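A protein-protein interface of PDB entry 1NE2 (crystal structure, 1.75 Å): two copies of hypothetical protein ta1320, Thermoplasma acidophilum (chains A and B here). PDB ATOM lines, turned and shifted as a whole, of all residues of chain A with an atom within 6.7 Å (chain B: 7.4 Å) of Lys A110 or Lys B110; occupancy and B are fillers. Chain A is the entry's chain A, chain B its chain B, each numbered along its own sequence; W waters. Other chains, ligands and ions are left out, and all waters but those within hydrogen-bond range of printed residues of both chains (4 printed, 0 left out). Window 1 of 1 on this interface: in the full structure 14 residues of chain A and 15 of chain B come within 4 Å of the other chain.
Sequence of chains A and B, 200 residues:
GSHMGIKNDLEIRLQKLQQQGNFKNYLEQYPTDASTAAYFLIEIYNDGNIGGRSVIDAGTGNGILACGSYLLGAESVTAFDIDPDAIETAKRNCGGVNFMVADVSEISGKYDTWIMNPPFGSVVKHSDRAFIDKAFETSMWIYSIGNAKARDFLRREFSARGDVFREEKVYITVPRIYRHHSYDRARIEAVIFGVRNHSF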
ATOM      1  N   GLY A  52      -5.623  -0.038  23.878  1.00  0.00           N
ATOM      2  CA  GLY A  52      -4.298  -0.100  24.476  1.00  0.00           C
ATOM      3  C   GLY A  52      -4.083  -1.319  25.355  1.00  0.00           C
ATOM      4  O   GLY A  52      -3.160  -1.351  26.167  1.00  0.00           O
ATOM      5  N   ARG A  53      -4.923  -2.335  25.189  1.00  0.00           N
ATOM      6  CA  ARG A  53      -4.807  -3.547  25.994  1.00  0.00           C
ATOM      7  C   ARG A  53      -4.467  -4.766  25.144  1.00  0.00           C
ATOM      8  O   ARG A  53      -4.602  -4.740  23.918  1.00  0.00           O
ATOM      9  CB  ARG A  53      -6.123  -3.814  26.739  1.00  0.00           C
ATOM     10  CG  ARG A  53      -6.573  -2.673  27.663  1.00  0.00           C
ATOM     11  CD  ARG A  53      -5.574  -2.466  28.793  1.00  0.00           C
ATOM     12  NE  ARG A  53      -6.014  -1.441  29.736  1.00  0.00           N
ATOM     13  CZ  ARG A  53      -5.921  -0.133  29.521  1.00  0.00           C
ATOM     14  NH1 ARG A  53      -5.398   0.325  28.390  1.00  0.00           N
ATOM     15  NH2 ARG A  53      -6.350   0.722  30.444  1.00  0.00           N
ATOM     16  N   SER A  54      -4.002  -5.825  25.802  1.00  0.00           N
ATOM     17  CA  SER A  54      -3.703  -7.081  25.111  1.00  0.00           C
ATOM     18  C   SER A  54      -4.976  -7.904  25.296  1.00  0.00           C
ATOM     19  O   SER A  54      -5.404  -8.177  26.423  1.00  0.00           O
ATOM     20  CB  SER A  54      -2.492  -7.779  25.743  1.00  0.00           C
ATOM     21  OG  SER A  54      -2.693  -8.019  27.126  1.00  0.00           O
ATOM     22  N   ILE A  56      -7.480 -11.354  24.180  1.00  0.00           N
ATOM     23  CA  ILE A  56      -7.532 -12.691  23.602  1.00  0.00           C
ATOM     24  C   ILE A  56      -9.003 -13.054  23.394  1.00  0.00           C
ATOM     25  O   ILE A  56      -9.824 -12.954  24.313  1.00  0.00           O
ATOM     26  CB  ILE A  56      -6.814 -13.778  24.463  1.00  0.00           C
ATOM     27  CG1 ILE A  56      -6.965 -15.134  23.768  1.00  0.00           C
ATOM     28  CG2 ILE A  56      -7.388 -13.835  25.890  1.00  0.00           C
ATOM     29  CD1 ILE A  56      -6.086 -16.244  24.338  1.00  0.00           C
ATOM     30  N   GLU A  75      -4.004  -2.913  21.881  1.00  0.00           N
ATOM     31  CA  GLU A  75      -2.568  -2.877  21.654  1.00  0.00           C
ATOM     32  C   GLU A  75      -2.139  -4.176  20.988  1.00  0.00           C
ATOM     33  O   GLU A  75      -1.264  -4.185  20.121  1.00  0.00           O
ATOM     34  CB  GLU A  75      -1.854  -2.697  22.982  1.00  0.00           C
ATOM     35  CG  GLU A  75      -0.351  -2.642  22.894  1.00  0.00           C
ATOM     36  CD  GLU A  75       0.238  -2.197  24.207  1.00  0.00           C
ATOM     37  OE1 GLU A  75       0.203  -0.977  24.488  1.00  0.00           O
ATOM     38  OE2 GLU A  75       0.700  -3.064  24.974  1.00  0.00           O
ATOM     39  N   SER A 108      -1.790 -20.678  27.144  1.00  0.00           N
ATOM     40  CA  SER A 108      -1.083 -20.506  28.406  1.00  0.00           C
ATOM     41  C   SER A 108      -0.562 -19.098  28.652  1.00  0.00           C
ATOM     42  O   SER A 108      -0.002 -18.826  29.709  1.00  0.00           O
ATOM     43  CB  SER A 108       0.074 -21.514  28.507  1.00  0.00           C
ATOM     44  OG  SER A 108       0.940 -21.429  27.387  1.00  0.00           O
ATOM     45  N   GLY A 109      -0.746 -18.199  27.692  1.00  0.00           N
ATOM     46  CA  GLY A 109      -0.254 -16.841  27.876  1.00  0.00           C
ATOM     47  C   GLY A 109      -1.133 -15.957  28.739  1.00  0.00           C
ATOM     48  O   GLY A 109      -2.271 -16.312  29.039  1.00  0.00           O
ATOM     49  N   LYS A 110      -0.594 -14.813  29.158  1.00  0.00           N
ATOM     50  CA  LYS A 110      -1.330 -13.855  29.983  1.00  0.00           C
ATOM     51  C   LYS A 110      -1.776 -12.676  29.123  1.00  0.00           C
ATOM     52  O   LYS A 110      -1.030 -12.209  28.253  1.00  0.00           O
ATOM     53  CB  LYS A 110      -0.451 -13.356  31.138  1.00  0.00           C
ATOM     54  CG  LYS A 110      -0.154 -14.406  32.209  1.00  0.00           C
ATOM     55  CD  LYS A 110      -1.409 -14.837  32.945  1.00  0.00           C
ATOM     56  CE  LYS A 110      -1.094 -15.768  34.110  1.00  0.00           C
ATOM     57  NZ  LYS A 110      -0.570 -17.094  33.680  1.00  0.00           N
ATOM     58  N   TYR A 111      -3.000 -12.212  29.370  1.00  0.00           N
ATOM     59  CA  TYR A 111      -3.610 -11.110  28.626  1.00  0.00           C
ATOM     60  C   TYR A 111      -4.431 -10.228  29.559  1.00  0.00           C
ATOM     61  O   TYR A 111      -4.889 -10.676  30.609  1.00  0.00           O
ATOM     62  CB  TYR A 111      -4.553 -11.671  27.553  1.00  0.00           C
ATOM     63  CG  TYR A 111      -3.864 -12.598  26.581  1.00  0.00           C
ATOM     64  CD1 TYR A 111      -3.264 -12.100  25.430  1.00  0.00           C
ATOM     65  CD2 TYR A 111      -3.738 -13.961  26.860  1.00  0.00           C
ATOM     66  CE1 TYR A 111      -2.543 -12.929  24.576  1.00  0.00           C
ATOM     67  CE2 TYR A 111      -3.011 -14.807  26.016  1.00  0.00           C
ATOM     68  CZ  TYR A 111      -2.418 -14.274  24.877  1.00  0.00           C
ATOM     69  OH  TYR A 111      -1.672 -15.077  24.053  1.00  0.00           O
ATOM     70  N   ASP A 112      -4.634  -8.976  29.170  1.00  0.00           N
ATOM     71  CA  ASP A 112      -5.454  -8.088  29.987  1.00  0.00           C
ATOM     72  C   ASP A 112      -6.898  -8.565  29.970  1.00  0.00           C
ATOM     73  O   ASP A 112      -7.546  -8.691  31.009  1.00  0.00           O
ATOM     74  CB  ASP A 112      -5.475  -6.662  29.425  1.00  0.00           C
ATOM     75  CG  ASP A 112      -4.180  -5.926  29.623  1.00  0.00           C
ATOM     76  OD1 ASP A 112      -3.818  -5.673  30.791  1.00  0.00           O
ATOM     77  OD2 ASP A 112      -3.536  -5.587  28.606  1.00  0.00           O
ATOM     78  N   PHE A 136      -9.869 -17.589  33.692  1.00  0.00           N
ATOM     79  CA  PHE A 136      -9.407 -17.182  35.018  1.00  0.00           C
ATOM     80  C   PHE A 136      -7.918 -17.443  35.235  1.00  0.00           C
ATOM     81  O   PHE A 136      -7.290 -16.846  36.107  1.00  0.00           O
ATOM     82  CB  PHE A 136     -10.225 -17.894  36.102  1.00  0.00           C
ATOM     83  CG  PHE A 136     -11.565 -17.261  36.365  1.00  0.00           C
ATOM     84  CD1 PHE A 136     -11.653 -15.936  36.786  1.00  0.00           C
ATOM     85  CD2 PHE A 136     -12.738 -17.988  36.200  1.00  0.00           C
ATOM     86  CE1 PHE A 136     -12.889 -15.345  37.038  1.00  0.00           C
ATOM     87  CE2 PHE A 136     -13.980 -17.408  36.451  1.00  0.00           C
ATOM     88  CZ  PHE A 136     -14.056 -16.084  36.870  1.00  0.00           C
ATOM     89  N   GLU A 137      -7.357 -18.340  34.436  1.00  0.00           N
ATOM     90  CA  GLU A 137      -5.943 -18.662  34.536  1.00  0.00           C
ATOM     91  C   GLU A 137      -5.120 -17.647  33.756  1.00  0.00           C
ATOM     92  O   GLU A 137      -3.960 -17.381  34.080  1.00  0.00           O
ATOM     93  CB  GLU A 137      -5.686 -20.051  33.940  1.00  0.00           C
ATOM     94  CG  GLU A 137      -4.216 -20.391  33.748  1.00  0.00           C
ATOM     95  CD  GLU A 137      -4.011 -21.559  32.798  1.00  0.00           C
ATOM     96  OE1 GLU A 137      -4.789 -22.535  32.878  1.00  0.00           O
ATOM     97  OE2 GLU A 137      -3.067 -21.505  31.979  1.00  0.00           O
ATOM     98  N   THR A 138      -5.734 -17.054  32.743  1.00  0.00           N
ATOM     99  CA  THR A 138      -5.007 -16.149  31.869  1.00  0.00           C
ATOM    100  C   THR A 138      -5.270 -14.653  31.845  1.00  0.00           C
ATOM    101  O   THR A 138      -4.355 -13.890  31.545  1.00  0.00           O
ATOM    102  CB  THR A 138      -5.149 -16.607  30.413  1.00  0.00           C
ATOM    103  OG1 THR A 138      -6.508 -16.440  30.007  1.00  0.00           O
ATOM    104  CG2 THR A 138      -4.766 -18.071  30.262  1.00  0.00           C
ATOM    105  N   SER A 139      -6.489 -14.225  32.154  1.00  0.00           N
ATOM    106  CA  SER A 139      -6.810 -12.807  32.042  1.00  0.00           C
ATOM    107  C   SER A 139      -7.381 -12.098  33.264  1.00  0.00           C
ATOM    108  O   SER A 139      -7.996 -12.714  34.134  1.00  0.00           O
ATOM    109  CB  SER A 139      -7.768 -12.628  30.865  1.00  0.00           C
ATOM    110  OG  SER A 139      -7.321 -13.376  29.740  1.00  0.00           O
ATOM    111  N   MET A 140      -7.180 -10.787  33.303  1.00  0.00           N
ATOM    112  CA  MET A 140      -7.659  -9.956  34.401  1.00  0.00           C
ATOM    113  C   MET A 140      -9.141  -9.629  34.243  1.00  0.00           C
ATOM    114  O   MET A 140      -9.887  -9.601  35.220  1.00  0.00           O
ATOM    115  CB  MET A 140      -6.851  -8.657  34.469  1.00  0.00           C
ATOM    116  CG  MET A 140      -7.449  -7.597  35.388  1.00  0.00           C
ATOM    117  SD  MET A 140      -7.604  -8.143  37.232  1.00  0.00           S
ATOM    118  CE  MET A 140      -6.700  -6.649  38.052  1.00  0.00           C
ATOM    119  N   PHE A 200      -4.519 -11.849  39.950  1.00  0.00           N
ATOM    120  CA  PHE A 200      -3.838 -10.732  39.304  1.00  0.00           C
ATOM    121  C   PHE A 200      -4.204  -9.405  39.963  1.00  0.00           C
ATOM    122  O   PHE A 200      -4.637  -8.489  39.237  1.00  0.00           O
ATOM    123  CB  PHE A 200      -4.202 -10.683  37.816  1.00  0.00           C
ATOM    124  CG  PHE A 200      -4.019 -11.990  37.102  1.00  0.00           C
ATOM    125  CD1 PHE A 200      -2.778 -12.620  37.081  1.00  0.00           C
ATOM    126  CD2 PHE A 200      -5.090 -12.595  36.451  1.00  0.00           C
ATOM    127  CE1 PHE A 200      -2.606 -13.835  36.422  1.00  0.00           C
ATOM    128  CE2 PHE A 200      -4.929 -13.810  35.789  1.00  0.00           C
ATOM    129  CZ  PHE A 200      -3.685 -14.431  35.774  1.00  0.00           C
ATOM    130  OXT PHE A 200      -4.048  -9.296  41.198  1.00  0.00           O
ATOM    131  N   GLY B  52       4.699 -20.621  24.544  1.00  0.00           N
ATOM    132  CA  GLY B  52       3.341 -20.497  25.050  1.00  0.00           C
ATOM    133  C   GLY B  52       3.090 -19.247  25.872  1.00  0.00           C
ATOM    134  O   GLY B  52       2.109 -19.166  26.607  1.00  0.00           O
ATOM    135  N   ARG B  53       3.970 -18.265  25.744  1.00  0.00           N
ATOM    136  CA  ARG B  53       3.835 -17.031  26.509  1.00  0.00           C
ATOM    137  C   ARG B  53       3.515 -15.836  25.636  1.00  0.00           C
ATOM    138  O   ARG B  53       3.726 -15.860  24.423  1.00  0.00           O
ATOM    139  CB  ARG B  53       5.145 -16.730  27.246  1.00  0.00           C
ATOM    140  CG  ARG B  53       5.674 -17.853  28.104  1.00  0.00           C
ATOM    141  CD  ARG B  53       4.716 -18.218  29.236  1.00  0.00           C
ATOM    142  NE  ARG B  53       5.368 -19.137  30.171  1.00  0.00           N
ATOM    143  CZ  ARG B  53       4.753 -19.781  31.160  1.00  0.00           C
ATOM    144  NH1 ARG B  53       3.452 -19.612  31.364  1.00  0.00           N
ATOM    145  NH2 ARG B  53       5.435 -20.617  31.935  1.00  0.00           N
ATOM    146  N   SER B  54       2.987 -14.786  26.257  1.00  0.00           N
ATOM    147  CA  SER B  54       2.734 -13.554  25.525  1.00  0.00           C
ATOM    148  C   SER B  54       4.025 -12.763  25.770  1.00  0.00           C
ATOM    149  O   SER B  54       4.459 -12.594  26.912  1.00  0.00           O
ATOM    150  CB  SER B  54       1.503 -12.828  26.081  1.00  0.00           C
ATOM    151  OG  SER B  54       1.606 -12.612  27.475  1.00  0.00           O
ATOM    152  N   VAL B  55       4.646 -12.298  24.695  1.00  0.00           N
ATOM    153  CA  VAL B  55       5.924 -11.598  24.785  1.00  0.00           C
ATOM    154  C   VAL B  55       5.899 -10.225  24.142  1.00  0.00           C
ATOM    155  O   VAL B  55       5.267 -10.031  23.111  1.00  0.00           O
ATOM    156  CB  VAL B  55       7.028 -12.422  24.064  1.00  0.00           C
ATOM    157  CG1 VAL B  55       8.361 -11.676  24.075  1.00  0.00           C
ATOM    158  CG2 VAL B  55       7.170 -13.785  24.723  1.00  0.00           C
ATOM    159  N   ILE B  56       6.597  -9.276  24.753  1.00  0.00           N
ATOM    160  CA  ILE B  56       6.706  -7.951  24.175  1.00  0.00           C
ATOM    161  C   ILE B  56       8.190  -7.601  24.103  1.00  0.00           C
ATOM    162  O   ILE B  56       8.925  -7.718  25.086  1.00  0.00           O
ATOM    163  CB  ILE B  56       5.933  -6.858  24.976  1.00  0.00           C
ATOM    164  CG1 ILE B  56       6.070  -5.518  24.237  1.00  0.00           C
ATOM    165  CG2 ILE B  56       6.434  -6.775  26.423  1.00  0.00           C
ATOM    166  CD1 ILE B  56       5.070  -4.450  24.682  1.00  0.00           C
ATOM    167  N   GLU B  75       3.339 -17.674  22.286  1.00  0.00           N
ATOM    168  CA  GLU B  75       1.923 -17.699  21.959  1.00  0.00           C
ATOM    169  C   GLU B  75       1.538 -16.427  21.209  1.00  0.00           C
ATOM    170  O   GLU B  75       0.740 -16.456  20.276  1.00  0.00           O
ATOM    171  CB  GLU B  75       1.107 -17.846  23.236  1.00  0.00           C
ATOM    172  CG  GLU B  75      -0.382 -17.981  23.004  1.00  0.00           C
ATOM    173  CD  GLU B  75      -1.084 -18.411  24.266  1.00  0.00           C
ATOM    174  OE1 GLU B  75      -0.987 -19.606  24.612  1.00  0.00           O
ATOM    175  OE2 GLU B  75      -1.706 -17.556  24.923  1.00  0.00           O
ATOM    176  N   SER B  76       2.104 -15.307  21.629  1.00  0.00           N
ATOM    177  CA  SER B  76       1.854 -14.033  20.966  1.00  0.00           C
ATOM    178  C   SER B  76       3.086 -13.171  21.151  1.00  0.00           C
ATOM    179  O   SER B  76       3.739 -13.229  22.193  1.00  0.00           O
ATOM    180  CB  SER B  76       0.617 -13.342  21.558  1.00  0.00           C
ATOM    181  OG  SER B  76       0.699 -13.245  22.966  1.00  0.00           O
ATOM    182  N   ILE B 107       2.974   2.345  25.718  1.00  0.00           N
ATOM    183  CA  ILE B 107       2.672   0.942  26.012  1.00  0.00           C
ATOM    184  C   ILE B 107       1.754   0.808  27.232  1.00  0.00           C
ATOM    185  O   ILE B 107       2.019   1.378  28.288  1.00  0.00           O
ATOM    186  CB  ILE B 107       3.977   0.141  26.218  1.00  0.00           C
ATOM    187  CG1 ILE B 107       4.846   0.224  24.953  1.00  0.00           C
ATOM    188  CG2 ILE B 107       3.659  -1.308  26.560  1.00  0.00           C
ATOM    189  CD1 ILE B 107       4.163  -0.260  23.677  1.00  0.00           C
ATOM    190  N   SER B 108       0.672   0.050  27.085  1.00  0.00           N
ATOM    191  CA  SER B 108      -0.286  -0.092  28.179  1.00  0.00           C
ATOM    192  C   SER B 108      -0.905  -1.471  28.372  1.00  0.00           C
ATOM    193  O   SER B 108      -1.795  -1.637  29.201  1.00  0.00           O
ATOM    194  CB  SER B 108      -1.403   0.944  28.004  1.00  0.00           C
ATOM    195  OG  SER B 108      -1.927   0.914  26.680  1.00  0.00           O
ATOM    196  N   GLY B 109      -0.452  -2.460  27.615  1.00  0.00           N
ATOM    197  CA  GLY B 109      -1.004  -3.794  27.776  1.00  0.00           C
ATOM    198  C   GLY B 109      -0.183  -4.650  28.723  1.00  0.00           C
ATOM    199  O   GLY B 109       0.879  -4.228  29.187  1.00  0.00           O
ATOM    200  N   LYS B 110      -0.682  -5.850  29.017  1.00  0.00           N
ATOM    201  CA  LYS B 110      -0.001  -6.795  29.904  1.00  0.00           C
ATOM    202  C   LYS B 110       0.566  -7.957  29.088  1.00  0.00           C
ATOM    203  O   LYS B 110      -0.094  -8.459  28.171  1.00  0.00           O
ATOM    204  CB  LYS B 110      -0.985  -7.334  30.950  1.00  0.00           C
ATOM    205  CG  LYS B 110      -0.436  -8.453  31.822  1.00  0.00           C
ATOM    206  CD  LYS B 110      -1.502  -8.962  32.792  1.00  0.00           C
ATOM    207  CE  LYS B 110      -0.991 -10.127  33.639  1.00  0.00           C
ATOM    208  NZ  LYS B 110       0.165  -9.757  34.507  1.00  0.00           N
ATOM    209  N   TYR B 111       1.783  -8.381  29.430  1.00  0.00           N
ATOM    210  CA  TYR B 111       2.472  -9.475  28.735  1.00  0.00           C
ATOM    211  C   TYR B 111       3.261 -10.315  29.741  1.00  0.00           C
ATOM    212  O   TYR B 111       3.739  -9.793  30.745  1.00  0.00           O
ATOM    213  CB  TYR B 111       3.452  -8.896  27.705  1.00  0.00           C
ATOM    214  CG  TYR B 111       2.793  -7.977  26.712  1.00  0.00           C
ATOM    215  CD1 TYR B 111       2.196  -8.490  25.567  1.00  0.00           C
ATOM    216  CD2 TYR B 111       2.685  -6.603  26.958  1.00  0.00           C
ATOM    217  CE1 TYR B 111       1.498  -7.673  24.686  1.00  0.00           C
ATOM    218  CE2 TYR B 111       1.981  -5.768  26.078  1.00  0.00           C
ATOM    219  CZ  TYR B 111       1.388  -6.321  24.942  1.00  0.00           C
ATOM    220  OH  TYR B 111       0.664  -5.548  24.060  1.00  0.00           O
ATOM    221  N   ASP B 112       3.411 -11.609  29.469  1.00  0.00           N
ATOM    222  CA  ASP B 112       4.173 -12.480  30.367  1.00  0.00           C
ATOM    223  C   ASP B 112       5.628 -12.051  30.498  1.00  0.00           C
ATOM    224  O   ASP B 112       6.174 -11.919  31.603  1.00  0.00           O
ATOM    225  CB  ASP B 112       4.206 -13.920  29.835  1.00  0.00           C
ATOM    226  CG  ASP B 112       2.899 -14.646  30.006  1.00  0.00           C
ATOM    227  OD1 ASP B 112       2.484 -14.860  31.159  1.00  0.00           O
ATOM    228  OD2 ASP B 112       2.291 -15.016  28.981  1.00  0.00           O
ATOM    229  N   THR B 113       6.244 -11.839  29.340  1.00  0.00           N
ATOM    230  CA  THR B 113       7.661 -11.536  29.243  1.00  0.00           C
ATOM    231  C   THR B 113       8.010 -10.263  28.487  1.00  0.00           C
ATOM    232  O   THR B 113       7.487 -10.014  27.406  1.00  0.00           O
ATOM    233  CB  THR B 113       8.358 -12.724  28.553  1.00  0.00           C
ATOM    234  OG1 THR B 113       7.996 -13.935  29.231  1.00  0.00           O
ATOM    235  CG2 THR B 113       9.873 -12.555  28.559  1.00  0.00           C
ATOM    236  N   GLU B 137       5.748  -2.361  34.972  1.00  0.00           N
ATOM    237  CA  GLU B 137       4.323  -2.091  35.038  1.00  0.00           C
ATOM    238  C   GLU B 137       3.619  -2.987  34.017  1.00  0.00           C
ATOM    239  O   GLU B 137       2.399  -3.157  34.054  1.00  0.00           O
ATOM    240  CB  GLU B 137       4.071  -0.618  34.697  1.00  0.00           C
ATOM    241  CG  GLU B 137       2.613  -0.222  34.608  1.00  0.00           C
ATOM    242  CD  GLU B 137       2.435   1.221  34.173  1.00  0.00           C
ATOM    243  OE1 GLU B 137       1.274   1.669  34.057  1.00  0.00           O
ATOM    244  OE2 GLU B 137       3.458   1.905  33.948  1.00  0.00           O
ATOM    245  N   THR B 138       4.414  -3.588  33.135  1.00  0.00           N
ATOM    246  CA  THR B 138       3.903  -4.409  32.037  1.00  0.00           C
ATOM    247  C   THR B 138       4.028  -5.933  32.106  1.00  0.00           C
ATOM    248  O   THR B 138       3.083  -6.656  31.758  1.00  0.00           O
ATOM    249  CB  THR B 138       4.577  -3.969  30.705  1.00  0.00           C
ATOM    250  OG1 THR B 138       4.322  -2.575  30.464  1.00  0.00           O
ATOM    251  CG2 THR B 138       4.046  -4.784  29.535  1.00  0.00           C
ATOM    252  N   SER B 139       5.180  -6.425  32.547  1.00  0.00           N
ATOM    253  CA  SER B 139       5.411  -7.865  32.542  1.00  0.00           C
ATOM    254  C   SER B 139       5.892  -8.527  33.824  1.00  0.00           C
ATOM    255  O   SER B 139       6.459  -7.885  34.705  1.00  0.00           O
ATOM    256  CB  SER B 139       6.402  -8.194  31.423  1.00  0.00           C
ATOM    257  OG  SER B 139       6.010  -7.582  30.206  1.00  0.00           O
ATOM    258  N   MET B 140       5.676  -9.837  33.895  1.00  0.00           N
ATOM    259  CA  MET B 140       6.078 -10.636  35.046  1.00  0.00           C
ATOM    260  C   MET B 140       7.559 -11.003  34.988  1.00  0.00           C
ATOM    261  O   MET B 140       8.245 -11.021  36.018  1.00  0.00           O
ATOM    262  CB  MET B 140       5.230 -11.907  35.113  1.00  0.00           C
ATOM    263  CG  MET B 140       5.625 -12.844  36.238  1.00  0.00           C
ATOM    264  SD  MET B 140       4.189 -14.020  36.768  1.00  0.00           S
ATOM    265  CE  MET B 140       4.465 -15.455  35.525  1.00  0.00           C
ATOM    266  N   PHE B 200       3.291  -8.661  39.756  1.00  0.00           N
ATOM    267  CA  PHE B 200       2.490  -9.803  39.332  1.00  0.00           C
ATOM    268  C   PHE B 200       3.343 -10.933  38.767  1.00  0.00           C
ATOM    269  O   PHE B 200       3.207 -11.234  37.562  1.00  0.00           O
ATOM    270  CB  PHE B 200       1.451  -9.358  38.296  1.00  0.00           C
ATOM    271  CG  PHE B 200       1.941  -8.283  37.366  1.00  0.00           C
ATOM    272  CD1 PHE B 200       3.068  -8.482  36.576  1.00  0.00           C
ATOM    273  CD2 PHE B 200       1.273  -7.065  37.283  1.00  0.00           C
ATOM    274  CE1 PHE B 200       3.524  -7.485  35.719  1.00  0.00           C
ATOM    275  CE2 PHE B 200       1.722  -6.062  36.429  1.00  0.00           C
ATOM    276  CZ  PHE B 200       2.850  -6.273  35.645  1.00  0.00           C
ATOM    277  OXT PHE B 200       4.138 -11.506  39.541  1.00  0.00           O
HETATM  278  O   HOH W   1       1.622 -17.347  31.143  1.00  0.00           O
HETATM  279  O   HOH W   2      -0.556 -10.372  26.343  1.00  0.00           O
HETATM  280  O   HOH W   3      -4.152   3.112  28.068  1.00  0.00           O
HETATM  281  O   HOH W   4      -2.598  -3.402  31.165  1.00  0.00           O
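The backbone carbonyl oxygen of Lys A110 lies within hydrogen-bond range of the side-chain hydroxyl of Ser B54, at 2.8 Å.
The backbone NH (N) of Lys A110 sits at hydrogen-bond distance from the side-chain carboxylate (OD2) of Asp B112 (2.9 Å).
The side-chain hydroxyl (OH) of Tyr A111 is in hydrogen-bond range of the side-chain hydroxyl (OG) of Ser B76, at 3.2 Å.
OE1 of Glu A75 is in hydrogen-bond range of N of Ser B108 (2.8 Å).
The side-chain carboxylate (OD2) of Asp A112 sits at hydrogen-bond distance from the backbone NH (N) of Lys B110.
The backbone carbonyl oxygen (O) of Gly A52 lies within hydrogen-bond range of the backbone NH (N) of Gly B109 (3.3 Å).
The side-chain carboxylate of Glu A75 is in hydrogen-bond range of the side-chain hydroxyl of Tyr B111.
OE2 of Glu B75 is in hydrogen-bond range of OH of Tyr A111 (2.6 Å).
N of Gly A109 sits at hydrogen-bond distance from O of Gly B52 (3.2 Å).
O of Gly A52 is in hydrogen-bond range of OG of Ser B108 (2.6 Å).
The side-chain hydroxyl (OG) of Ser A108 lies within hydrogen-bond range of the backbone carbonyl oxygen (O) of Gly B52, 2.7 Å away.
The backbone carbonyl oxygen of Lys B110 sits at hydrogen-bond distance from the side-chain hydroxyl of Ser A54 (2.8 Å).
N of Gly A109 sits at hydrogen-bond distance from OE2 of Glu B75 (3.0 Å).
The side-chain carboxylate (OE1) of Glu B75 lies within hydrogen-bond range of the backbone NH (N) of Ser A108 (2.9 Å).
OE2 of Glu A75 lies within hydrogen-bond range of N of Gly B109, 2.9 Å away.
N of Val B55 sits at hydrogen-bond distance from O of Ser B76.
The backbone NH of Ser A54 is in hydrogen-bond range of the side-chain carboxylate of Asp A112, 2.9 Å away.
The backbone NH (N) of Ser B54 lies within hydrogen-bond range of the side-chain carboxylate (OD2) of Asp B112, at 2.8 Å.
The backbone carbonyl oxygen (O) of Asp B112 lies within hydrogen-bond range of the backbone NH (N) of Met B140 (3.1 Å).
The backbone carbonyl oxygen of Arg B53 lies within hydrogen-bond range of the backbone NH of Ser B76 (3.3 Å).
N of Met A140 sits at hydrogen-bond distance from O of Asp A112 (3.1 Å).
Among the printed residues, merely in contact across the chains: Asp A112 with Gly B109 (3.2 Å), Gly A109 with Asp B112 (3.3 Å), Glu A75 with Ile B107 (3.5 Å), Lys A110 with Lys B110 (3.9 Å), Arg A53 with Ser B108 (3.9 Å) and Ser A108 with Arg B53 (3.9 Å).
Of chain B, only Ser B54 (2.8 Å), Lys B110 (3.9 Å) and Asp B112 (2.9 Å) come within 4 Å of Lys A110.
Lys B110 touches three residues of chain A.
Printed residues of chain B within 4 Å of Arg A53: Ser B108 (3.9 Å).
Of the printed residues of chain A, Gly B52 touches Ser A108 (2.7 Å) and Gly A109 (3.2 Å).
Printed residues of chain A within 4 Å of Ser B54: Lys A110 (2.8 Å).
Printed residues of chain A within 4 Å of Ser B76: Tyr A111.
The nearest residue of chain B that does not touch Lys A110 is Tyr B111 (4.5 Å).
The nearest residue of chain A that does not touch Lys B110 is Tyr A111 (4.4 Å).
The nearest printed residue of chain A that does not touch Arg B53 is Gly A109 (4.3 Å).
Of the 19 printed residues of chain B, 11 touch a printed residue of chain A.
Hydrophobic or aromatic side chains of chain B within 4 Å of the printed part of chain A: Ile B107 and Tyr B111.
Hydrophobic or aromatic side chains of chain A within 4 Å of the printed part of chain B: Tyr A111.
Along chain A the printed residues that touch a printed residue of chain B span positions 52 to 112.
Among the printed residues, no Asp or Glu carboxylate lies within 4 Å of a Lys or Arg side-chain nitrogen of the other chain.
Glu A75 touches Ser B108, and with the chains exchanged Ser A108 touches Glu B75.
Glu A75 touches Tyr B111, and with the chains exchanged Tyr A111 touches Glu B75.
Gly A109 touches Asp B112, and with the chains exchanged Asp A112 touches Gly B109.
Lys A110 touches its own counterpart, Lys B110.
Positions printed for both chains: 52, 53, 54, 56, 75, 108, 109, 110, 111, 112, 137, 138, 139, 140 and 200.
Of the 21 pairs that touch across the chains among the printed residues, 19 have their exchanged pair printed and touching as well.
Water W4 bridges the side-chain carboxylate of Asp A112 and the backbone carbonyl oxygen of Ser B108.
Water W1 lies within hydrogen-bond range of the backbone carbonyl oxygen of Ser A108 (2.6 Å), the side-chain carboxylate of Asp B112 (2.6 Å), the guanidinium group of Arg B53 (2.9 Å) and the side-chain amino group of Lys A110 (3.4 Å).
Water W2 lies within hydrogen-bond range of the backbone carbonyl oxygen (O) of Lys B110 (2.7 Å), the backbone carbonyl oxygen (O) of Lys A110 (2.7 Å), the side-chain hydroxyl (OG) of Ser A54 (3.3 Å) and the side-chain hydroxyl (OG) of Ser B54 (3.3 Å).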
